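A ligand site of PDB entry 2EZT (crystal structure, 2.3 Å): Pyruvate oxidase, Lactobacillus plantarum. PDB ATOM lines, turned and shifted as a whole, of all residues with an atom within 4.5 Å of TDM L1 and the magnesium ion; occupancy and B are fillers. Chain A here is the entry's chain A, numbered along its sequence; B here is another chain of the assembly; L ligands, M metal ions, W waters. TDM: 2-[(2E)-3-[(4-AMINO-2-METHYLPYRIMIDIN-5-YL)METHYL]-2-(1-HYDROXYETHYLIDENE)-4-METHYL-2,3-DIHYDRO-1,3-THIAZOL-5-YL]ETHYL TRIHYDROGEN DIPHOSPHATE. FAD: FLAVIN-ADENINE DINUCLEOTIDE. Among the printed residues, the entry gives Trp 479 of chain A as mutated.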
ATOM      1  N   ASN A  92     -22.618  10.333 -19.472  1.00  0.00           N
ATOM      2  CA  ASN A  92     -23.291  10.224 -18.175  1.00  0.00           C
ATOM      3  C   ASN A  92     -22.940  11.343 -17.262  1.00  0.00           C
ATOM      4  O   ASN A  92     -23.777  11.788 -16.452  1.00  0.00           O
ATOM      5  CB  ASN A  92     -23.033   8.883 -17.471  1.00  0.00           C
ATOM      6  CG  ASN A  92     -23.972   7.808 -17.945  1.00  0.00           C
ATOM      7  OD1 ASN A  92     -24.090   7.569 -19.156  1.00  0.00           O
ATOM      8  ND2 ASN A  92     -24.662   7.151 -17.012  1.00  0.00           N
ATOM      9  N   VAL A 394     -25.361   6.353  -5.996  1.00  0.00           N
ATOM     10  CA  VAL A 394     -26.796   6.296  -6.254  1.00  0.00           C
ATOM     11  C   VAL A 394     -27.325   4.897  -5.863  1.00  0.00           C
ATOM     12  O   VAL A 394     -26.784   3.897  -6.295  1.00  0.00           O
ATOM     13  CB  VAL A 394     -27.087   6.629  -7.738  1.00  0.00           C
ATOM     14  CG1 VAL A 394     -28.527   6.286  -8.126  1.00  0.00           C
ATOM     15  CG2 VAL A 394     -26.788   8.101  -8.023  1.00  0.00           C
ATOM     16  N   GLY A 395     -28.368   4.859  -5.038  1.00  0.00           N
ATOM     17  CA  GLY A 395     -28.985   3.612  -4.583  1.00  0.00           C
ATOM     18  C   GLY A 395     -29.413   3.761  -3.133  1.00  0.00           C
ATOM     19  O   GLY A 395     -29.713   4.865  -2.679  1.00  0.00           O
ATOM     20  N   ASP A 396     -29.436   2.643  -2.387  1.00  0.00           N
ATOM     21  CA  ASP A 396     -29.778   2.697  -0.952  1.00  0.00           C
ATOM     22  C   ASP A 396     -29.003   3.740  -0.157  1.00  0.00           C
ATOM     23  O   ASP A 396     -29.534   4.302   0.805  1.00  0.00           O
ATOM     24  CB  ASP A 396     -29.608   1.342  -0.294  1.00  0.00           C
ATOM     25  CG  ASP A 396     -30.794   0.442  -0.467  1.00  0.00           C
ATOM     26  OD1 ASP A 396     -31.852   0.917  -0.940  1.00  0.00           O
ATOM     27  OD2 ASP A 396     -30.661  -0.753  -0.143  1.00  0.00           O
ATOM     28  N   ILE A 397     -27.757   4.010  -0.578  1.00  0.00           N
ATOM     29  CA  ILE A 397     -26.866   4.937   0.111  1.00  0.00           C
ATOM     30  C   ILE A 397     -27.411   6.350   0.208  1.00  0.00           C
ATOM     31  O   ILE A 397     -27.152   7.036   1.207  1.00  0.00           O
ATOM     32  CB  ILE A 397     -25.399   4.984  -0.506  1.00  0.00           C
ATOM     33  CG1 ILE A 397     -24.448   5.810   0.392  1.00  0.00           C
ATOM     34  CG2 ILE A 397     -25.398   5.539  -1.956  1.00  0.00           C
ATOM     35  CD1 ILE A 397     -24.255   5.251   1.829  1.00  0.00           C
ATOM     36  N   ALA A 420     -29.353  11.175 -11.695  1.00  0.00           N
ATOM     37  CA  ALA A 420     -29.145  10.030 -10.793  1.00  0.00           C
ATOM     38  C   ALA A 420     -28.329   8.893 -11.439  1.00  0.00           C
ATOM     39  O   ALA A 420     -28.699   7.719 -11.389  1.00  0.00           O
ATOM     40  CB  ALA A 420     -30.494   9.500 -10.221  1.00  0.00           C
ATOM     41  N   THR A 421     -27.195   9.266 -12.039  1.00  0.00           N
ATOM     42  CA  THR A 421     -26.287   8.261 -12.573  1.00  0.00           C
ATOM     43  C   THR A 421     -25.422   7.618 -11.492  1.00  0.00           C
ATOM     44  O   THR A 421     -24.730   8.289 -10.707  1.00  0.00           O
ATOM     45  CB  THR A 421     -25.389   8.825 -13.736  1.00  0.00           C
ATOM     46  OG1 THR A 421     -24.546   7.784 -14.227  1.00  0.00           O
ATOM     47  CG2 THR A 421     -24.490  10.014 -13.269  1.00  0.00           C
ATOM     48  N   MET A 422     -25.456   6.290 -11.470  1.00  0.00           N
ATOM     49  CA  MET A 422     -24.549   5.491 -10.655  1.00  0.00           C
ATOM     50  C   MET A 422     -23.113   5.724 -11.069  1.00  0.00           C
ATOM     51  O   MET A 422     -22.830   6.025 -12.240  1.00  0.00           O
ATOM     52  CB  MET A 422     -24.880   4.004 -10.781  1.00  0.00           C
ATOM     53  CG  MET A 422     -26.119   3.574 -10.029  1.00  0.00           C
ATOM     54  SD  MET A 422     -26.676   1.979 -10.637  1.00  0.00           S
ATOM     55  CE  MET A 422     -25.386   0.924  -9.980  1.00  0.00           C
ATOM     56  N   GLY A 446     -22.704   2.242  -3.047  1.00  0.00           N
ATOM     57  CA  GLY A 446     -23.123   0.847  -3.128  1.00  0.00           C
ATOM     58  C   GLY A 446     -22.160   0.069  -4.004  1.00  0.00           C
ATOM     59  O   GLY A 446     -21.352   0.660  -4.764  1.00  0.00           O
ATOM     60  N   ASP A 447     -22.234  -1.264  -3.904  1.00  0.00           N
ATOM     61  CA  ASP A 447     -21.360  -2.101  -4.721  1.00  0.00           C
ATOM     62  C   ASP A 447     -21.630  -2.022  -6.236  1.00  0.00           C
ATOM     63  O   ASP A 447     -20.681  -2.075  -7.027  1.00  0.00           O
ATOM     64  CB  ASP A 447     -21.275  -3.549  -4.210  1.00  0.00           C
ATOM     65  CG  ASP A 447     -22.621  -4.221  -4.016  1.00  0.00           C
ATOM     66  OD1 ASP A 447     -23.685  -3.612  -4.227  1.00  0.00           O
ATOM     67  OD2 ASP A 447     -22.610  -5.399  -3.620  1.00  0.00           O
ATOM     68  N   GLY A 448     -22.890  -1.871  -6.640  1.00  0.00           N
ATOM     69  CA  GLY A 448     -23.240  -1.697  -8.036  1.00  0.00           C
ATOM     70  C   GLY A 448     -22.660  -0.431  -8.632  1.00  0.00           C
ATOM     71  O   GLY A 448     -22.076  -0.458  -9.732  1.00  0.00           O
ATOM     72  N   GLY A 449     -22.843   0.689  -7.934  1.00  0.00           N
ATOM     73  CA  GLY A 449     -22.270   1.960  -8.362  1.00  0.00           C
ATOM     74  C   GLY A 449     -20.758   2.060  -8.277  1.00  0.00           C
ATOM     75  O   GLY A 449     -20.126   2.580  -9.184  1.00  0.00           O
ATOM     76  N   MET A 452     -19.143   0.371 -11.326  1.00  0.00           N
ATOM     77  CA  MET A 452     -19.189   1.025 -12.619  1.00  0.00           C
ATOM     78  C   MET A 452     -17.965   1.898 -12.881  1.00  0.00           C
ATOM     79  O   MET A 452     -17.525   1.990 -14.037  1.00  0.00           O
ATOM     80  CB  MET A 452     -20.485   1.803 -12.767  1.00  0.00           C
ATOM     81  CG  MET A 452     -21.680   0.861 -12.858  1.00  0.00           C
ATOM     82  SD  MET A 452     -23.157   1.777 -13.203  1.00  0.00           S
ATOM     83  CE  MET A 452     -24.338   0.456 -13.571  1.00  0.00           C
ATOM     84  N   PHE A 472     -20.653  -0.291   0.131  1.00  0.00           N
ATOM     85  CA  PHE A 472     -21.720  -1.014   0.845  1.00  0.00           C
ATOM     86  C   PHE A 472     -22.088  -2.260   0.042  1.00  0.00           C
ATOM     87  O   PHE A 472     -22.901  -2.195  -0.871  1.00  0.00           O
ATOM     88  CB  PHE A 472     -22.942  -0.109   1.091  1.00  0.00           C
ATOM     89  CG  PHE A 472     -22.654   1.045   2.026  1.00  0.00           C
ATOM     90  CD1 PHE A 472     -21.838   2.116   1.609  1.00  0.00           C
ATOM     91  CD2 PHE A 472     -23.166   1.045   3.325  1.00  0.00           C
ATOM     92  CE1 PHE A 472     -21.527   3.166   2.499  1.00  0.00           C
ATOM     93  CE2 PHE A 472     -22.901   2.116   4.208  1.00  0.00           C
ATOM     94  CZ  PHE A 472     -22.067   3.176   3.797  1.00  0.00           C
ATOM     95  N   ASN A 474     -23.828  -5.385  -0.637  1.00  0.00           N
ATOM     96  CA  ASN A 474     -24.979  -6.242  -0.345  1.00  0.00           C
ATOM     97  C   ASN A 474     -25.184  -7.337  -1.397  1.00  0.00           C
ATOM     98  O   ASN A 474     -26.076  -8.187  -1.245  1.00  0.00           O
ATOM     99  CB  ASN A 474     -26.266  -5.394  -0.124  1.00  0.00           C
ATOM    100  CG  ASN A 474     -26.525  -4.431  -1.250  1.00  0.00           C
ATOM    101  OD1 ASN A 474     -25.850  -4.476  -2.270  1.00  0.00           O
ATOM    102  ND2 ASN A 474     -27.493  -3.555  -1.076  1.00  0.00           N
ATOM    103  N   GLN A 476     -26.332  -6.882  -4.306  1.00  0.00           N
ATOM    104  CA  GLN A 476     -27.624  -6.573  -4.911  1.00  0.00           C
ATOM    105  C   GLN A 476     -27.578  -5.179  -5.455  1.00  0.00           C
ATOM    106  O   GLN A 476     -26.744  -4.374  -5.073  1.00  0.00           O
ATOM    107  CB  GLN A 476     -28.775  -6.635  -3.885  1.00  0.00           C
ATOM    108  CG  GLN A 476     -28.850  -7.877  -3.010  1.00  0.00           C
ATOM    109  CD  GLN A 476     -29.812  -7.728  -1.841  1.00  0.00           C
ATOM    110  OE1 GLN A 476     -30.219  -8.710  -1.243  1.00  0.00           O
ATOM    111  NE2 GLN A 476     -30.184  -6.496  -1.529  1.00  0.00           N
ATOM    112  N   TYR A 477     -28.490  -4.910  -6.390  1.00  0.00           N
ATOM    113  CA  TYR A 477     -28.954  -3.568  -6.632  1.00  0.00           C
ATOM    114  C   TYR A 477     -30.155  -3.439  -5.682  1.00  0.00           C
ATOM    115  O   TYR A 477     -31.308  -3.716  -6.074  1.00  0.00           O
ATOM    116  CB  TYR A 477     -29.401  -3.456  -8.091  1.00  0.00           C
ATOM    117  CG  TYR A 477     -28.278  -3.615  -9.109  1.00  0.00           C
ATOM    118  CD1 TYR A 477     -27.122  -2.800  -9.046  1.00  0.00           C
ATOM    119  CD2 TYR A 477     -28.370  -4.545 -10.147  1.00  0.00           C
ATOM    120  CE1 TYR A 477     -26.089  -2.934  -9.964  1.00  0.00           C
ATOM    121  CE2 TYR A 477     -27.339  -4.683 -11.099  1.00  0.00           C
ATOM    122  CZ  TYR A 477     -26.187  -3.878 -10.994  1.00  0.00           C
ATOM    123  OH  TYR A 477     -25.169  -4.015 -11.917  1.00  0.00           O
ATOM    124  N   GLY A 478     -29.897  -3.083  -4.429  1.00  0.00           N
ATOM    125  CA  GLY A 478     -30.930  -3.172  -3.388  1.00  0.00           C
ATOM    126  C   GLY A 478     -32.106  -2.255  -3.694  1.00  0.00           C
ATOM    127  O   GLY A 478     -33.282  -2.668  -3.582  1.00  0.00           O
ATOM    128  N   TRP A 479     -31.779  -1.017  -4.095  1.00  0.00           N
ATOM    129  CA  TRP A 479     -32.760  -0.020  -4.501  1.00  0.00           C
ATOM    130  C   TRP A 479     -33.766  -0.585  -5.490  1.00  0.00           C
ATOM    131  O   TRP A 479     -34.978  -0.396  -5.318  1.00  0.00           O
ATOM    132  CB  TRP A 479     -32.038   1.182  -5.118  1.00  0.00           C
ATOM    133  CG  TRP A 479     -32.857   2.462  -5.231  1.00  0.00           C
ATOM    134  CD1 TRP A 479     -33.351   3.006  -6.356  1.00  0.00           C
ATOM    135  CD2 TRP A 479     -33.208   3.374  -4.155  1.00  0.00           C
ATOM    136  NE1 TRP A 479     -34.007   4.183  -6.083  1.00  0.00           N
ATOM    137  CE2 TRP A 479     -33.913   4.441  -4.740  1.00  0.00           C
ATOM    138  CE3 TRP A 479     -32.986   3.386  -2.773  1.00  0.00           C
ATOM    139  CZ2 TRP A 479     -34.434   5.522  -3.988  1.00  0.00           C
ATOM    140  CZ3 TRP A 479     -33.496   4.455  -2.008  1.00  0.00           C
ATOM    141  CH2 TRP A 479     -34.206   5.509  -2.632  1.00  0.00           C
ATOM    142  N   ILE A 480     -33.259  -1.297  -6.513  1.00  0.00           N
ATOM    143  CA  ILE A 480     -34.095  -1.912  -7.567  1.00  0.00           C
ATOM    144  C   ILE A 480     -34.771  -3.239  -7.145  1.00  0.00           C
ATOM    145  O   ILE A 480     -35.899  -3.553  -7.573  1.00  0.00           O
ATOM    146  CB  ILE A 480     -33.263  -2.131  -8.873  1.00  0.00           C
ATOM    147  CG1 ILE A 480     -32.536  -0.849  -9.268  1.00  0.00           C
ATOM    148  CG2 ILE A 480     -34.164  -2.639 -10.014  1.00  0.00           C
ATOM    149  CD1 ILE A 480     -33.435   0.378  -9.341  1.00  0.00           C
ATOM    150  N   ILE B  32     -29.110  -3.949 -17.290  1.00  0.00           N
ATOM    151  CA  ILE B  32     -29.203  -3.726 -15.847  1.00  0.00           C
ATOM    152  C   ILE B  32     -30.599  -3.214 -15.552  1.00  0.00           C
ATOM    153  O   ILE B  32     -31.081  -2.322 -16.228  1.00  0.00           O
ATOM    154  CB  ILE B  32     -28.116  -2.702 -15.354  1.00  0.00           C
ATOM    155  CG1 ILE B  32     -26.717  -3.326 -15.511  1.00  0.00           C
ATOM    156  CG2 ILE B  32     -28.408  -2.178 -13.936  1.00  0.00           C
ATOM    157  CD1 ILE B  32     -25.590  -2.459 -15.109  1.00  0.00           C
ATOM    158  N   PRO B  33     -31.274  -3.809 -14.546  1.00  0.00           N
ATOM    159  CA  PRO B  33     -32.666  -3.391 -14.257  1.00  0.00           C
ATOM    160  C   PRO B  33     -32.760  -2.010 -13.616  1.00  0.00           C
ATOM    161  O   PRO B  33     -31.789  -1.526 -13.046  1.00  0.00           O
ATOM    162  CB  PRO B  33     -33.151  -4.453 -13.266  1.00  0.00           C
ATOM    163  CG  PRO B  33     -31.905  -4.905 -12.589  1.00  0.00           C
ATOM    164  CD  PRO B  33     -30.800  -4.843 -13.606  1.00  0.00           C
ATOM    165  N   GLY B  34     -33.932  -1.388 -13.736  1.00  0.00           N
ATOM    166  CA  GLY B  34     -34.293  -0.219 -12.968  1.00  0.00           C
ATOM    167  C   GLY B  34     -35.802  -0.164 -12.922  1.00  0.00           C
ATOM    168  O   GLY B  34     -36.449  -0.878 -13.703  1.00  0.00           O
ATOM    169  N   GLU B  59     -23.801  -0.915 -18.255  1.00  0.00           N
ATOM    170  CA  GLU B  59     -24.605  -1.056 -19.496  1.00  0.00           C
ATOM    171  C   GLU B  59     -23.808  -0.977 -20.800  1.00  0.00           C
ATOM    172  O   GLU B  59     -24.263  -1.538 -21.790  1.00  0.00           O
ATOM    173  CB  GLU B  59     -25.846  -0.126 -19.544  1.00  0.00           C
ATOM    174  CG  GLU B  59     -26.807  -0.283 -18.339  1.00  0.00           C
ATOM    175  CD  GLU B  59     -26.386   0.561 -17.124  1.00  0.00           C
ATOM    176  OE1 GLU B  59     -25.212   1.035 -17.039  1.00  0.00           O
ATOM    177  OE2 GLU B  59     -27.251   0.763 -16.245  1.00  0.00           O
ATOM    178  N   SER B  82     -31.931   1.251 -18.320  1.00  0.00           N
ATOM    179  CA  SER B  82     -33.022   1.965 -17.658  1.00  0.00           C
ATOM    180  C   SER B  82     -33.015   3.458 -18.050  1.00  0.00           C
ATOM    181  O   SER B  82     -32.067   3.961 -18.677  1.00  0.00           O
ATOM    182  CB  SER B  82     -32.876   1.812 -16.145  1.00  0.00           C
ATOM    183  OG  SER B  82     -31.531   2.098 -15.786  1.00  0.00           O
ATOM    184  N   PRO B  85     -29.464   7.544 -17.198  1.00  0.00           N
ATOM    185  CA  PRO B  85     -28.082   6.999 -17.160  1.00  0.00           C
ATOM    186  C   PRO B  85     -27.908   5.553 -17.627  1.00  0.00           C
ATOM    187  O   PRO B  85     -26.862   5.193 -18.119  1.00  0.00           O
ATOM    188  CB  PRO B  85     -27.713   7.129 -15.678  1.00  0.00           C
ATOM    189  CG  PRO B  85     -28.978   7.182 -14.960  1.00  0.00           C
ATOM    190  CD  PRO B  85     -29.889   7.970 -15.861  1.00  0.00           C
ATOM    191  N   GLY B  86     -28.936   4.721 -17.484  1.00  0.00           N
ATOM    192  CA  GLY B  86     -28.862   3.328 -17.959  1.00  0.00           C
ATOM    193  C   GLY B  86     -28.642   3.266 -19.453  1.00  0.00           C
ATOM    194  O   GLY B  86     -27.714   2.604 -19.929  1.00  0.00           O
ATOM    195  N   HIS B  89     -25.389   5.015 -20.928  1.00  0.00           N
ATOM    196  CA  HIS B  89     -24.252   4.090 -20.800  1.00  0.00           C
ATOM    197  C   HIS B  89     -24.092   3.149 -22.004  1.00  0.00           C
ATOM    198  O   HIS B  89     -22.990   2.656 -22.248  1.00  0.00           O
ATOM    199  CB  HIS B  89     -24.363   3.231 -19.532  1.00  0.00           C
ATOM    200  CG  HIS B  89     -23.570   3.752 -18.364  1.00  0.00           C
ATOM    201  ND1 HIS B  89     -23.657   3.184 -17.119  1.00  0.00           N
ATOM    202  CD2 HIS B  89     -22.692   4.776 -18.259  1.00  0.00           C
ATOM    203  CE1 HIS B  89     -22.839   3.811 -16.293  1.00  0.00           C
ATOM    204  NE2 HIS B  89     -22.252   4.788 -16.956  1.00  0.00           N
ATOM    205  N   PHE B 121     -38.488  12.511 -11.524  1.00  0.00           N
ATOM    206  CA  PHE B 121     -37.168  11.986 -11.242  1.00  0.00           C
ATOM    207  C   PHE B 121     -36.610  11.164 -12.404  1.00  0.00           C
ATOM    208  O   PHE B 121     -37.275  10.244 -12.905  1.00  0.00           O
ATOM    209  CB  PHE B 121     -37.274  11.142  -9.982  1.00  0.00           C
ATOM    210  CG  PHE B 121     -36.028  10.414  -9.652  1.00  0.00           C
ATOM    211  CD1 PHE B 121     -34.954  11.076  -9.081  1.00  0.00           C
ATOM    212  CD2 PHE B 121     -35.911   9.064  -9.908  1.00  0.00           C
ATOM    213  CE1 PHE B 121     -33.794  10.403  -8.773  1.00  0.00           C
ATOM    214  CE2 PHE B 121     -34.751   8.391  -9.599  1.00  0.00           C
ATOM    215  CZ  PHE B 121     -33.700   9.051  -9.010  1.00  0.00           C
ATOM    216  N   GLN B 122     -35.396  11.512 -12.858  1.00  0.00           N
ATOM    217  CA  GLN B 122     -34.730  10.784 -13.955  1.00  0.00           C
ATOM    218  C   GLN B 122     -35.605  10.756 -15.226  1.00  0.00           C
ATOM    219  O   GLN B 122     -35.454   9.879 -16.083  1.00  0.00           O
ATOM    220  CB  GLN B 122     -34.428   9.352 -13.508  1.00  0.00           C
ATOM    221  CG  GLN B 122     -33.141   8.745 -13.948  1.00  0.00           C
ATOM    222  CD  GLN B 122     -32.718   7.591 -13.019  1.00  0.00           C
ATOM    223  OE1 GLN B 122     -33.556   6.851 -12.534  1.00  0.00           O
ATOM    224  NE2 GLN B 122     -31.439   7.468 -12.766  1.00  0.00           N
HETATM  225  O1A TDM L   1     -25.494  -1.659  -5.350  1.00  0.00           O
HETATM  226  PA  TDM L   1     -26.097  -0.309  -5.668  1.00  0.00           P
HETATM  227  O2A TDM L   1     -25.169   0.781  -6.087  1.00  0.00           O
HETATM  228  O3A TDM L   1     -26.850   0.228  -4.361  1.00  0.00           O
HETATM  229  PB  TDM L   1     -27.684  -0.529  -3.216  1.00  0.00           P
HETATM  230  O2B TDM L   1     -27.041   0.016  -1.928  1.00  0.00           O
HETATM  231  O3B TDM L   1     -27.519  -2.039  -3.365  1.00  0.00           O
HETATM  232  O1B TDM L   1     -29.065   0.033  -3.459  1.00  0.00           O
HETATM  233  O7  TDM L   1     -27.231  -0.403  -6.756  1.00  0.00           O
HETATM  234  C7  TDM L   1     -27.925   0.782  -7.170  1.00  0.00           C
HETATM  235  C6  TDM L   1     -29.162   0.248  -7.868  1.00  0.00           C
HETATM  236  C5  TDM L   1     -29.784   1.229  -8.853  1.00  0.00           C
HETATM  237  S1  TDM L   1     -30.420   2.714  -8.173  1.00  0.00           S
HETATM  238  C2  TDM L   1     -30.975   3.209  -9.778  1.00  0.00           C
HETATM  239  C27 TDM L   1     -31.697   4.528  -9.831  1.00  0.00           C
HETATM  240  C29 TDM L   1     -31.927   5.339  -8.583  1.00  0.00           C
HETATM  241  O28 TDM L   1     -32.141   5.064 -10.974  1.00  0.00           O
HETATM  242  N3  TDM L   1     -30.628   2.287 -10.749  1.00  0.00           N
HETATM  243  C4  TDM L   1     -29.972   1.186 -10.245  1.00  0.00           C
HETATM  244  CM4 TDM L   1     -29.515   0.011 -11.086  1.00  0.00           C
HETATM  245  C7' TDM L   1     -30.891   2.448 -12.199  1.00  0.00           C
HETATM  246  C5' TDM L   1     -29.558   2.891 -12.863  1.00  0.00           C
HETATM  247  C4' TDM L   1     -28.970   4.155 -12.632  1.00  0.00           C
HETATM  248  N4' TDM L   1     -29.515   5.087 -11.812  1.00  0.00           N
HETATM  249  N3' TDM L   1     -27.800   4.481 -13.256  1.00  0.00           N
HETATM  250  C2' TDM L   1     -27.193   3.613 -14.104  1.00  0.00           C
HETATM  251  CM2 TDM L   1     -25.903   4.024 -14.745  1.00  0.00           C
HETATM  252  N1' TDM L   1     -27.728   2.395 -14.344  1.00  0.00           N
HETATM  253  C6' TDM L   1     -28.888   2.031 -13.744  1.00  0.00           C
HETATM  254  PA  FAD L   2     -33.126  21.704  -7.695  1.00  0.00           P
HETATM  255  O1A FAD L   2     -31.714  22.017  -8.130  1.00  0.00           O
HETATM  256  O2A FAD L   2     -33.973  20.813  -8.566  1.00  0.00           O
HETATM  257  O5B FAD L   2     -33.908  23.092  -7.463  1.00  0.00           O
HETATM  258  C5B FAD L   2     -33.308  24.248  -6.891  1.00  0.00           C
HETATM  259  C4B FAD L   2     -34.354  25.339  -7.033  1.00  0.00           C
HETATM  260  O4B FAD L   2     -33.918  26.523  -6.359  1.00  0.00           O
HETATM  261  C3B FAD L   2     -34.602  25.748  -8.488  1.00  0.00           C
HETATM  262  O3B FAD L   2     -36.014  25.834  -8.673  1.00  0.00           O
HETATM  263  C2B FAD L   2     -33.927  27.119  -8.619  1.00  0.00           C
HETATM  264  O2B FAD L   2     -34.549  27.973  -9.570  1.00  0.00           O
HETATM  265  C1B FAD L   2     -34.093  27.657  -7.220  1.00  0.00           C
HETATM  266  N9A FAD L   2     -33.054  28.650  -6.838  1.00  0.00           N
HETATM  267  C8A FAD L   2     -31.748  28.615  -7.134  1.00  0.00           C
HETATM  268  N7A FAD L   2     -31.139  29.672  -6.561  1.00  0.00           N
HETATM  269  C5A FAD L   2     -32.085  30.390  -5.894  1.00  0.00           C
HETATM  270  C6A FAD L   2     -32.068  31.562  -5.118  1.00  0.00           C
HETATM  271  N6A FAD L   2     -30.919  32.278  -4.913  1.00  0.00           N
HETATM  272  N1A FAD L   2     -33.231  31.995  -4.573  1.00  0.00           N
HETATM  273  C2A FAD L   2     -34.386  31.323  -4.766  1.00  0.00           C
HETATM  274  N3A FAD L   2     -34.428  30.187  -5.504  1.00  0.00           N
HETATM  275  C4A FAD L   2     -33.302  29.717  -6.066  1.00  0.00           C
HETATM  276  N1  FAD L   2     -35.064  13.984  -3.315  1.00  0.00           N
HETATM  277  C2  FAD L   2     -36.018  14.007  -2.356  1.00  0.00           C
HETATM  278  O2  FAD L   2     -36.222  15.066  -1.708  1.00  0.00           O
HETATM  279  N3  FAD L   2     -36.744  12.889  -2.105  1.00  0.00           N
HETATM  280  C4  FAD L   2     -36.536  11.737  -2.806  1.00  0.00           C
HETATM  281  O4  FAD L   2     -37.218  10.721  -2.553  1.00  0.00           O
HETATM  282  C4X FAD L   2     -35.543  11.697  -3.781  1.00  0.00           C
HETATM  283  N5  FAD L   2     -35.272  10.573  -4.529  1.00  0.00           N
HETATM  284  C5X FAD L   2     -33.975  10.468  -5.019  1.00  0.00           C
HETATM  285  C6  FAD L   2     -33.373   9.227  -5.269  1.00  0.00           C
HETATM  286  C7  FAD L   2     -32.061   9.141  -5.739  1.00  0.00           C
HETATM  287  C7M FAD L   2     -31.488   7.759  -5.975  1.00  0.00           C
HETATM  288  C8  FAD L   2     -31.310  10.327  -5.953  1.00  0.00           C
HETATM  289  C8M FAD L   2     -29.884  10.307  -6.466  1.00  0.00           C
HETATM  290  C9  FAD L   2     -31.914  11.562  -5.691  1.00  0.00           C
HETATM  291  C9A FAD L   2     -33.235  11.645  -5.231  1.00  0.00           C
HETATM  292  N10 FAD L   2     -33.853  12.840  -4.974  1.00  0.00           N
HETATM  293  C10 FAD L   2     -34.804  12.850  -4.014  1.00  0.00           C
HETATM  294  C1' FAD L   2     -33.157  14.103  -5.249  1.00  0.00           C
HETATM  295  C2' FAD L   2     -34.164  14.687  -6.304  1.00  0.00           C
HETATM  296  O2' FAD L   2     -34.233  13.940  -7.536  1.00  0.00           O
HETATM  297  C3' FAD L   2     -34.073  16.187  -6.654  1.00  0.00           C
HETATM  298  O3' FAD L   2     -32.800  16.506  -7.247  1.00  0.00           O
HETATM  299  C4' FAD L   2     -34.391  17.086  -5.444  1.00  0.00           C
HETATM  300  O4' FAD L   2     -35.513  16.606  -4.678  1.00  0.00           O
HETATM  301  C5' FAD L   2     -34.676  18.525  -5.851  1.00  0.00           C
HETATM  302  O5' FAD L   2     -34.005  19.346  -4.888  1.00  0.00           O
HETATM  303  P   FAD L   2     -33.933  20.944  -4.947  1.00  0.00           P
HETATM  304  O1P FAD L   2     -35.287  21.520  -5.235  1.00  0.00           O
HETATM  305  O2P FAD L   2     -33.172  21.316  -3.706  1.00  0.00           O
HETATM  306  O3P FAD L   2     -32.935  21.077  -6.220  1.00  0.00           O
HETATM  307 MG    MG M   1     -25.648  -3.004  -3.799  1.00  0.00          MG
HETATM  308  O   HOH W   1     -24.685   3.032  -4.881  1.00  0.00           O
HETATM  309  O   HOH W   2     -24.897  -1.603  -2.246  1.00  0.00           O
HETATM  310  O   HOH W   3     -31.870   4.673 -14.630  1.00  0.00           O
HETATM  311  O   HOH W   4     -26.077   2.417  -2.448  1.00  0.00           O
HETATM  312  O   HOH W   5     -26.613  -0.168   0.830  1.00  0.00           O
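Three residues have an atom within 4 Å of the magnesium ion: Asp 447, Asn 474 and Gln 476. Along chain A the residues within 4 Å of the magnesium ion span positions 447 to 476. The nearest printed residue that does not touch the magnesium ion is Phe 472 (4.1 Å).
Val 394 touches TDM L1. Gly 395 touches TDM L1 (CA to O1B, 3.8 Å). Gly 446 touches TDM L1. Met 452 touches TDM L1. Tyr 477 touches TDM L1. CG1 of Ile 480 touches C4 of TDM L1 (3.4 Å). Ile 32 of chain B touches TDM L1 (CG2 to CM4, 3.8 Å). Pro 33 of chain B touches TDM L1. OG of Ser 82 of chain B touches C6' of TDM L1 (3.3 Å). Pro 85 of chain B touches TDM L1. CA of Gly 86 of chain B touches N1' of TDM L1, 3.9 Å away. ND1 of His 89 of chain B touches CM2 of TDM L1 (3.4 Å). Hydrophobic or aromatic side chains within 4 Å of TDM L1: Val 394, Met 422, Met 452, Tyr 477, Trp 479, Ile 480, Ile 32 of chain B, Pro 85 of chain B and His 89 of chain B. Within 4 Å of TDM L1: Val 394, Gly 395, Asp 396, Ala 420, Met 422, Gly 446, Asp 447, Gly 448, Gly 449, Met 452, Asn 474, Gln 476, Tyr 477, Gly 478, Trp 479, Ile 480, Ile 32 of chain B, Pro 33 of chain B, Glu 59 of chain B, Ser 82 of chain B, Pro 85 of chain B, Gly 86 of chain B, His 89 of chain B and Gln 122 of chain B. The nearest printed residue that does not touch TDM L1 is Thr 421 (4.03 Å).
An oxygen (O2A) of TDM L1 is in hydrogen-bond range of the backbone NH (N) of Gly 449 (3.0 Å). N of Trp 479 lies within hydrogen-bond range of O1B of TDM L1, 3.0 Å away. The backbone NH of Met 422 sits at hydrogen-bond distance from a nitrogen (N3') of TDM L1, at 3.5 Å. The side-chain carboxylate of Glu 59 of chain B is in hydrogen-bond range of a nitrogen (N1') of TDM L1, at 2.6 Å. The backbone NH of Gly 448 sits close to an oxygen (O1A) of TDM L1. The backbone NH (N) of Asp 396 sits at hydrogen-bond distance from an oxygen (O1B) of TDM L1 (2.8 Å). O of Ala 420 sits at hydrogen-bond distance from N4' of TDM L1 (2.8 Å). The side-chain amide oxygen of Gln 122 of chain B sits at hydrogen-bond distance from an oxygen (O28) of TDM L1, 2.8 Å away. The backbone NH of Gly 478 lies within hydrogen-bond range of an oxygen (O1B) of TDM L1 (3.4 Å).
The magnesium ion is bound by O1A of TDM L1, OD1 of Asp 447, OD1 of Asn 474, O3B of TDM L1, O of Gln 476 and water W2. The magnesium ion has six donor atoms within binding distance.
OE1 of Glu 59 of chain B is in hydrogen-bond range of ND1 of His 89 of chain B (2.7 Å). The backbone NH (N) of Asp 447 sits at hydrogen-bond distance from the backbone carbonyl oxygen (O) of Phe 472 (3.2 Å). The backbone NH (N) of His 89 of chain B sits close to the side-chain amide oxygen (OD1) of Asn 92 (3.4 Å). The backbone carbonyl oxygen (O) of Ala 420 lies within hydrogen-bond range of the side-chain amide nitrogen (NE2) of Gln 122 of chain B (3.1 Å). The side-chain amide nitrogen (ND2) of Asn 92 sits at hydrogen-bond distance from the backbone carbonyl oxygen (O) of Pro 85 of chain B, at 3.1 Å.
Water W2 lies within hydrogen-bond range of the backbone carbonyl oxygen (O) of Phe 472, an oxygen (O2B) of TDM L1, the backbone NH (N) of Asp 447 and the side-chain amide nitrogen (ND2) of Asn 474. Water W1 lies within hydrogen-bond range of an oxygen (O2A) of TDM L1 (2.6 Å), the backbone carbonyl oxygen of Val 394 (2.7 Å) and the backbone NH of Gly 446 (2.8 Å). Water W3 bridges OG of Ser 82 of chain B (2.8 Å) and NE2 of Gln 122 of chain B (3.4 Å).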
